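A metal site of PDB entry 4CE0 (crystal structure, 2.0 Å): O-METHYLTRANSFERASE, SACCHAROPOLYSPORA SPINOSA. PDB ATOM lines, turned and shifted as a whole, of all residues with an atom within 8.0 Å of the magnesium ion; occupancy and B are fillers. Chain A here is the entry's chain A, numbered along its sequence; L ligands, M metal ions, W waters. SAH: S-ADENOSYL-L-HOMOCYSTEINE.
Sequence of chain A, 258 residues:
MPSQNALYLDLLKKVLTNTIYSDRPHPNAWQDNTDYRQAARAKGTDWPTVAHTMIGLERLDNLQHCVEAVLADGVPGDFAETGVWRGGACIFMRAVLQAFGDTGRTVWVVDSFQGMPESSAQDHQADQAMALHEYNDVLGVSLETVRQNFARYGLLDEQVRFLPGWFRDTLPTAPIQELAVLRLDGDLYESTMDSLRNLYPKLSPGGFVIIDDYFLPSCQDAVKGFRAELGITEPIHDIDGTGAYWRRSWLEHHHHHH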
ATOM      1  N   TRP A  47       0.568 -23.793 -15.892  1.00  0.00           N
ATOM      2  CA  TRP A  47       1.399 -22.599 -15.675  1.00  0.00           C
ATOM      3  C   TRP A  47       2.914 -22.887 -15.761  1.00  0.00           C
ATOM      4  O   TRP A  47       3.437 -23.630 -14.929  1.00  0.00           O
ATOM      5  CB  TRP A  47       1.155 -21.992 -14.304  1.00  0.00           C
ATOM      6  CG  TRP A  47      -0.282 -21.980 -13.776  1.00  0.00           C
ATOM      7  CD1 TRP A  47      -0.726 -22.528 -12.598  1.00  0.00           C
ATOM      8  CD2 TRP A  47      -1.437 -21.383 -14.406  1.00  0.00           C
ATOM      9  NE1 TRP A  47      -2.087 -22.307 -12.455  1.00  0.00           N
ATOM     10  CE2 TRP A  47      -2.537 -21.616 -13.546  1.00  0.00           C
ATOM     11  CE3 TRP A  47      -1.646 -20.697 -15.613  1.00  0.00           C
ATOM     12  CZ2 TRP A  47      -3.823 -21.177 -13.858  1.00  0.00           C
ATOM     13  CZ3 TRP A  47      -2.922 -20.275 -15.909  1.00  0.00           C
ATOM     14  CH2 TRP A  47      -3.989 -20.518 -15.034  1.00  0.00           C
ATOM     15  N   MET A  54       2.937 -16.965 -20.402  1.00  0.00           N
ATOM     16  CA  MET A  54       2.250 -18.230 -20.543  1.00  0.00           C
ATOM     17  C   MET A  54       1.681 -18.403 -21.960  1.00  0.00           C
ATOM     18  O   MET A  54       1.148 -19.463 -22.302  1.00  0.00           O
ATOM     19  CB  MET A  54       1.149 -18.353 -19.462  1.00  0.00           C
ATOM     20  CG  MET A  54      -0.103 -17.524 -19.707  1.00  0.00           C
ATOM     21  SD  MET A  54      -1.412 -17.874 -18.507  1.00  0.00           S
ATOM     22  CE  MET A  54      -0.759 -17.207 -16.971  1.00  0.00           C
ATOM     23  N   ILE A  55       1.854 -17.397 -22.825  1.00  0.00           N
ATOM     24  CA  ILE A  55       1.173 -17.458 -24.126  1.00  0.00           C
ATOM     25  C   ILE A  55       1.777 -18.339 -25.205  1.00  0.00           C
ATOM     26  O   ILE A  55       1.132 -18.570 -26.215  1.00  0.00           O
ATOM     27  CB  ILE A  55       0.867 -16.032 -24.714  1.00  0.00           C
ATOM     28  CG1 ILE A  55       2.127 -15.388 -25.252  1.00  0.00           C
ATOM     29  CG2 ILE A  55       0.163 -15.197 -23.684  1.00  0.00           C
ATOM     30  CD1 ILE A  55       1.912 -14.054 -25.996  1.00  0.00           C
ATOM     31  N   ARG A  59       1.735 -17.518 -30.171  1.00  0.00           N
ATOM     32  CA  ARG A  59       1.088 -16.234 -29.875  1.00  0.00           C
ATOM     33  C   ARG A  59       2.108 -15.068 -29.753  1.00  0.00           C
ATOM     34  O   ARG A  59       1.804 -13.924 -30.038  1.00  0.00           O
ATOM     35  CB  ARG A  59       0.156 -16.389 -28.683  1.00  0.00           C
ATOM     36  CG  ARG A  59      -0.899 -17.496 -28.936  1.00  0.00           C
ATOM     37  CD  ARG A  59      -2.231 -17.218 -28.311  1.00  0.00           C
ATOM     38  NE  ARG A  59      -2.225 -17.258 -26.851  1.00  0.00           N
ATOM     39  CZ  ARG A  59      -2.306 -18.375 -26.131  1.00  0.00           C
ATOM     40  NH1 ARG A  59      -2.362 -19.565 -26.717  1.00  0.00           N
ATOM     41  NH2 ARG A  59      -2.346 -18.303 -24.817  1.00  0.00           N
ATOM     42  N   GLU A  81      -1.276  -3.946 -22.913  1.00  0.00           N
ATOM     43  CA  GLU A  81      -1.827  -5.265 -22.573  1.00  0.00           C
ATOM     44  C   GLU A  81      -2.592  -5.216 -21.261  1.00  0.00           C
ATOM     45  O   GLU A  81      -2.082  -4.789 -20.220  1.00  0.00           O
ATOM     46  CB  GLU A  81      -0.772  -6.392 -22.538  1.00  0.00           C
ATOM     47  CG  GLU A  81      -1.442  -7.816 -22.385  1.00  0.00           C
ATOM     48  CD  GLU A  81      -0.457  -8.935 -22.109  1.00  0.00           C
ATOM     49  OE1 GLU A  81       0.492  -8.694 -21.313  1.00  0.00           O
ATOM     50  OE2 GLU A  81      -0.639 -10.053 -22.676  1.00  0.00           O
ATOM     51  N   GLY A  83      -3.880  -7.462 -18.754  1.00  0.00           N
ATOM     52  CA  GLY A  83      -3.633  -8.800 -18.233  1.00  0.00           C
ATOM     53  C   GLY A  83      -2.219  -9.230 -18.616  1.00  0.00           C
ATOM     54  O   GLY A  83      -1.988  -9.713 -19.734  1.00  0.00           O
ATOM     55  N   ARG A 183      -3.791  -5.568 -26.594  1.00  0.00           N
ATOM     56  CA  ARG A 183      -3.769  -7.007 -26.312  1.00  0.00           C
ATOM     57  C   ARG A 183      -4.591  -7.301 -25.063  1.00  0.00           C
ATOM     58  O   ARG A 183      -4.376  -6.701 -24.015  1.00  0.00           O
ATOM     59  CB  ARG A 183      -2.340  -7.516 -26.177  1.00  0.00           C
ATOM     60  CG  ARG A 183      -2.248  -9.032 -26.109  1.00  0.00           C
ATOM     61  CD  ARG A 183      -0.800  -9.575 -26.109  1.00  0.00           C
ATOM     62  NE  ARG A 183      -0.927 -10.897 -26.671  1.00  0.00           N
ATOM     63  CZ  ARG A 183      -1.281 -11.972 -25.995  1.00  0.00           C
ATOM     64  NH1 ARG A 183      -1.419 -11.950 -24.669  1.00  0.00           N
ATOM     65  NH2 ARG A 183      -1.456 -13.104 -26.673  1.00  0.00           N
ATOM     66  N   LEU A 184      -5.595  -8.175 -25.208  1.00  0.00           N
ATOM     67  CA  LEU A 184      -6.499  -8.545 -24.102  1.00  0.00           C
ATOM     68  C   LEU A 184      -6.154  -9.934 -23.629  1.00  0.00           C
ATOM     69  O   LEU A 184      -6.184 -10.905 -24.416  1.00  0.00           O
ATOM     70  CB  LEU A 184      -7.948  -8.493 -24.515  1.00  0.00           C
ATOM     71  CG  LEU A 184      -8.674  -7.167 -24.452  1.00  0.00           C
ATOM     72  CD1 LEU A 184      -8.051  -6.149 -25.362  1.00  0.00           C
ATOM     73  CD2 LEU A 184     -10.104  -7.412 -24.836  1.00  0.00           C
ATOM     74  N   ASP A 185      -5.770 -10.035 -22.377  1.00  0.00           N
ATOM     75  CA  ASP A 185      -5.428 -11.325 -21.820  1.00  0.00           C
ATOM     76  C   ASP A 185      -5.900 -11.359 -20.385  1.00  0.00           C
ATOM     77  O   ASP A 185      -5.187 -11.782 -19.494  1.00  0.00           O
ATOM     78  CB  ASP A 185      -3.918 -11.586 -21.937  1.00  0.00           C
ATOM     79  CG  ASP A 185      -3.578 -13.071 -21.919  1.00  0.00           C
ATOM     80  OD1 ASP A 185      -4.489 -13.904 -21.639  1.00  0.00           O
ATOM     81  OD2 ASP A 185      -2.388 -13.420 -22.203  1.00  0.00           O
ATOM     82  N   GLY A 186      -7.097 -10.829 -20.173  1.00  0.00           N
ATOM     83  CA  GLY A 186      -7.881 -11.131 -18.984  1.00  0.00           C
ATOM     84  C   GLY A 186      -8.874 -12.173 -19.452  1.00  0.00           C
ATOM     85  O   GLY A 186      -9.512 -12.019 -20.494  1.00  0.00           O
ATOM     86  N   ASP A 187      -9.001 -13.265 -18.714  1.00  0.00           N
ATOM     87  CA  ASP A 187      -9.855 -14.356 -19.155  1.00  0.00           C
ATOM     88  C   ASP A 187     -11.346 -14.073 -19.002  1.00  0.00           C
ATOM     89  O   ASP A 187     -12.170 -14.558 -19.777  1.00  0.00           O
ATOM     90  CB  ASP A 187      -9.483 -15.601 -18.365  1.00  0.00           C
ATOM     91  CG  ASP A 187      -8.081 -16.084 -18.689  1.00  0.00           C
ATOM     92  OD1 ASP A 187      -7.786 -16.274 -19.892  1.00  0.00           O
ATOM     93  OD2 ASP A 187      -7.271 -16.249 -17.747  1.00  0.00           O
ATOM     94  N   ILE A 211      -6.946 -10.959 -29.041  1.00  0.00           N
ATOM     95  CA  ILE A 211      -7.749 -11.593 -27.986  1.00  0.00           C
ATOM     96  C   ILE A 211      -7.060 -12.917 -27.625  1.00  0.00           C
ATOM     97  O   ILE A 211      -7.126 -13.878 -28.377  1.00  0.00           O
ATOM     98  CB  ILE A 211      -9.168 -11.890 -28.458  1.00  0.00           C
ATOM     99  CG1 ILE A 211      -9.815 -10.673 -29.114  1.00  0.00           C
ATOM    100  CG2 ILE A 211     -10.007 -12.375 -27.278  1.00  0.00           C
ATOM    101  CD1 ILE A 211     -10.168  -9.547 -28.155  1.00  0.00           C
ATOM    102  N   ASP A 212      -6.416 -12.982 -26.466  1.00  0.00           N
ATOM    103  CA  ASP A 212      -5.530 -14.093 -26.237  1.00  0.00           C
ATOM    104  C   ASP A 212      -6.300 -15.409 -26.070  1.00  0.00           C
ATOM    105  O   ASP A 212      -5.778 -16.454 -26.402  1.00  0.00           O
ATOM    106  CB  ASP A 212      -4.616 -13.844 -25.025  1.00  0.00           C
ATOM    107  CG  ASP A 212      -3.529 -14.896 -24.888  1.00  0.00           C
ATOM    108  OD1 ASP A 212      -2.566 -14.837 -25.685  1.00  0.00           O
ATOM    109  OD2 ASP A 212      -3.647 -15.792 -24.028  1.00  0.00           O
ATOM    110  N   ASP A 213      -7.525 -15.328 -25.534  1.00  0.00           N
ATOM    111  CA  ASP A 213      -8.341 -16.504 -25.239  1.00  0.00           C
ATOM    112  C   ASP A 213      -9.716 -16.415 -25.871  1.00  0.00           C
ATOM    113  O   ASP A 213     -10.739 -16.701 -25.232  1.00  0.00           O
ATOM    114  CB  ASP A 213      -8.519 -16.679 -23.725  1.00  0.00           C
ATOM    115  CG  ASP A 213      -7.234 -17.033 -23.046  1.00  0.00           C
ATOM    116  OD1 ASP A 213      -6.890 -18.236 -23.022  1.00  0.00           O
ATOM    117  OD2 ASP A 213      -6.550 -16.105 -22.555  1.00  0.00           O
ATOM    118  N   TYR A 214      -9.735 -16.043 -27.141  1.00  0.00           N
ATOM    119  CA  TYR A 214     -10.994 -15.905 -27.858  1.00  0.00           C
ATOM    120  C   TYR A 214     -11.897 -17.135 -27.779  1.00  0.00           C
ATOM    121  O   TYR A 214     -13.094 -17.019 -27.973  1.00  0.00           O
ATOM    122  CB  TYR A 214     -10.737 -15.630 -29.327  1.00  0.00           C
ATOM    123  CG  TYR A 214     -12.008 -15.473 -30.122  1.00  0.00           C
ATOM    124  CD1 TYR A 214     -12.990 -14.570 -29.742  1.00  0.00           C
ATOM    125  CD2 TYR A 214     -12.231 -16.235 -31.254  1.00  0.00           C
ATOM    126  CE1 TYR A 214     -14.175 -14.435 -30.479  1.00  0.00           C
ATOM    127  CE2 TYR A 214     -13.398 -16.118 -32.011  1.00  0.00           C
ATOM    128  CZ  TYR A 214     -14.374 -15.217 -31.618  1.00  0.00           C
ATOM    129  OH  TYR A 214     -15.513 -15.078 -32.352  1.00  0.00           O
ATOM    130  N   LEU A 216     -12.233 -19.220 -25.272  1.00  0.00           N
ATOM    131  CA  LEU A 216     -12.758 -19.329 -23.946  1.00  0.00           C
ATOM    132  C   LEU A 216     -14.149 -18.727 -24.002  1.00  0.00           C
ATOM    133  O   LEU A 216     -14.277 -17.563 -24.414  1.00  0.00           O
ATOM    134  CB  LEU A 216     -11.853 -18.540 -22.976  1.00  0.00           C
ATOM    135  CG  LEU A 216     -12.100 -18.675 -21.477  1.00  0.00           C
ATOM    136  CD1 LEU A 216     -11.632 -20.053 -21.013  1.00  0.00           C
ATOM    137  CD2 LEU A 216     -11.418 -17.552 -20.653  1.00  0.00           C
ATOM    138  N   CYS A 219     -14.672 -14.985 -22.462  1.00  0.00           N
ATOM    139  CA  CYS A 219     -13.929 -13.986 -23.226  1.00  0.00           C
ATOM    140  C   CYS A 219     -14.660 -13.772 -24.530  1.00  0.00           C
ATOM    141  O   CYS A 219     -14.930 -12.633 -24.935  1.00  0.00           O
ATOM    142  CB  CYS A 219     -12.452 -14.391 -23.396  1.00  0.00           C
ATOM    143  SG  CYS A 219     -11.502 -13.363 -24.539  1.00  0.00           S
ATOM    144  N   THR A 242      -6.661 -20.846 -30.118  1.00  0.00           N
ATOM    145  CA  THR A 242      -6.859 -20.312 -28.775  1.00  0.00           C
ATOM    146  C   THR A 242      -7.080 -18.787 -28.859  1.00  0.00           C
ATOM    147  O   THR A 242      -8.128 -18.278 -28.507  1.00  0.00           O
ATOM    148  CB  THR A 242      -5.644 -20.590 -27.881  1.00  0.00           C
ATOM    149  OG1 THR A 242      -5.550 -21.999 -27.659  1.00  0.00           O
ATOM    150  CG2 THR A 242      -5.747 -19.862 -26.522  1.00  0.00           C
ATOM    151  N   GLY A 243      -6.057 -18.085 -29.345  1.00  0.00           N
ATOM    152  CA  GLY A 243      -6.090 -16.666 -29.531  1.00  0.00           C
ATOM    153  C   GLY A 243      -6.651 -16.313 -30.889  1.00  0.00           C
ATOM    154  O   GLY A 243      -6.650 -17.110 -31.831  1.00  0.00           O
HETATM  155  N   SAH L   1       1.365 -14.596 -19.488  1.00  0.00           N
HETATM  156  CA  SAH L   1       0.046 -13.988 -19.735  1.00  0.00           C
HETATM  157  CB  SAH L   1      -0.686 -13.455 -18.528  1.00  0.00           C
HETATM  158  CG  SAH L   1      -2.144 -13.008 -18.462  1.00  0.00           C
HETATM  159  SD  SAH L   1      -2.806 -13.886 -17.014  1.00  0.00           S
HETATM  160  C   SAH L   1       0.490 -12.865 -20.580  1.00  0.00           C
HETATM  161  O   SAH L   1      -0.318 -11.969 -20.729  1.00  0.00           O
HETATM  162  OXT SAH L   1       1.777 -13.139 -21.023  1.00  0.00           O
HETATM  163  C5' SAH L   1      -4.246 -12.848 -16.572  1.00  0.00           C
HETATM  164  C4' SAH L   1      -3.882 -11.511 -15.921  1.00  0.00           C
HETATM  165  O4' SAH L   1      -4.998 -10.632 -15.950  1.00  0.00           O
HETATM  166  C3' SAH L   1      -3.499 -11.599 -14.442  1.00  0.00           C
HETATM  167  O3' SAH L   1      -2.212 -11.039 -14.311  1.00  0.00           O
HETATM  168  C2' SAH L   1      -4.558 -10.827 -13.645  1.00  0.00           C
HETATM  169  O2' SAH L   1      -4.135 -10.128 -12.454  1.00  0.00           O
HETATM  170  C1' SAH L   1      -5.117  -9.910 -14.727  1.00  0.00           C
HETATM  171  N9  SAH L   1      -6.532  -9.498 -14.586  1.00  0.00           N
HETATM  172  C8  SAH L   1      -7.627 -10.248 -14.958  1.00  0.00           C
HETATM  173  N7  SAH L   1      -8.725  -9.513 -14.745  1.00  0.00           N
HETATM  174  C5  SAH L   1      -8.367  -8.298 -14.274  1.00  0.00           C
HETATM  175  C6  SAH L   1      -9.071  -7.159 -13.885  1.00  0.00           C
HETATM  176  N6  SAH L   1     -10.410  -7.122 -13.948  1.00  0.00           N
HETATM  177  N1  SAH L   1      -8.405  -6.055 -13.423  1.00  0.00           N
HETATM  178  C2  SAH L   1      -7.019  -6.034 -13.355  1.00  0.00           C
HETATM  179  N3  SAH L   1      -6.338  -7.168 -13.709  1.00  0.00           N
HETATM  180  C4  SAH L   1      -6.986  -8.270 -14.203  1.00  0.00           C
HETATM  181 MG    MG M   1      -4.510 -15.859 -22.231  1.00  0.00          MG
HETATM  182  O   HOH W   1      -2.597 -16.294 -21.310  1.00  0.00           O
HETATM  183  O   HOH W   2      -5.108 -16.346 -20.299  1.00  0.00           O
HETATM  184  O   HOH W   3      -4.365 -18.137 -22.225  1.00  0.00           O
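The guanidinium group (NE) of Arg 59 lies within salt-bridge range of the side-chain carboxylate (OD1) of Asp 212 (2.7 Å). OD2 of Asp 185 is in salt-bridge range of NH1 of Arg 183, at 3.0 Å. N of Asp 212 sits at hydrogen-bond distance from O of Leu 184. N of Gly 243 lies close to O of Asp 212. OD1 of Asp 212 lies within salt-bridge range of NH1 of Arg 183. The backbone carbonyl oxygen of Asp 213 lies close to the side-chain sulfur of Cys 219, 3.5 Å away.
Of the 19 residues printed, 3 come within 4 Å of the magnesium ion.
Water W1 lies within hydrogen-bond range of the side-chain carboxylate of Asp 185 (3.0 Å) and the side-chain sulfur of Met 54 (3.4 Å). Water W3 lies within hydrogen-bond range of the side-chain carboxylate (OD1) of Asp 213 (2.6 Å) and the guanidinium group (NH2) of Arg 59 (3.3 Å).
The backbone carbonyl oxygen of Gly 83 lies close to an oxygen (O) of the ligand (3.0 Å). An oxygen (O) of the ligand lies close to the side-chain carboxylate (OD2) of Asp 185 (2.9 Å). A nitrogen (N) of the ligand lies close to the backbone NH of Met 54, 3.0 Å away. The side-chain carboxylate of Glu 81 lies close to an oxygen (O) of the ligand (2.8 Å).
The magnesium ion is bound by OD2 of Asp 212 (2.0 Å), OD1 of Asp 185 (2.0 Å), water W2 (2.1 Å), OD2 of Asp 213 (2.1 Å), water W1 (2.2 Å) and water W3 (2.3 Å).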
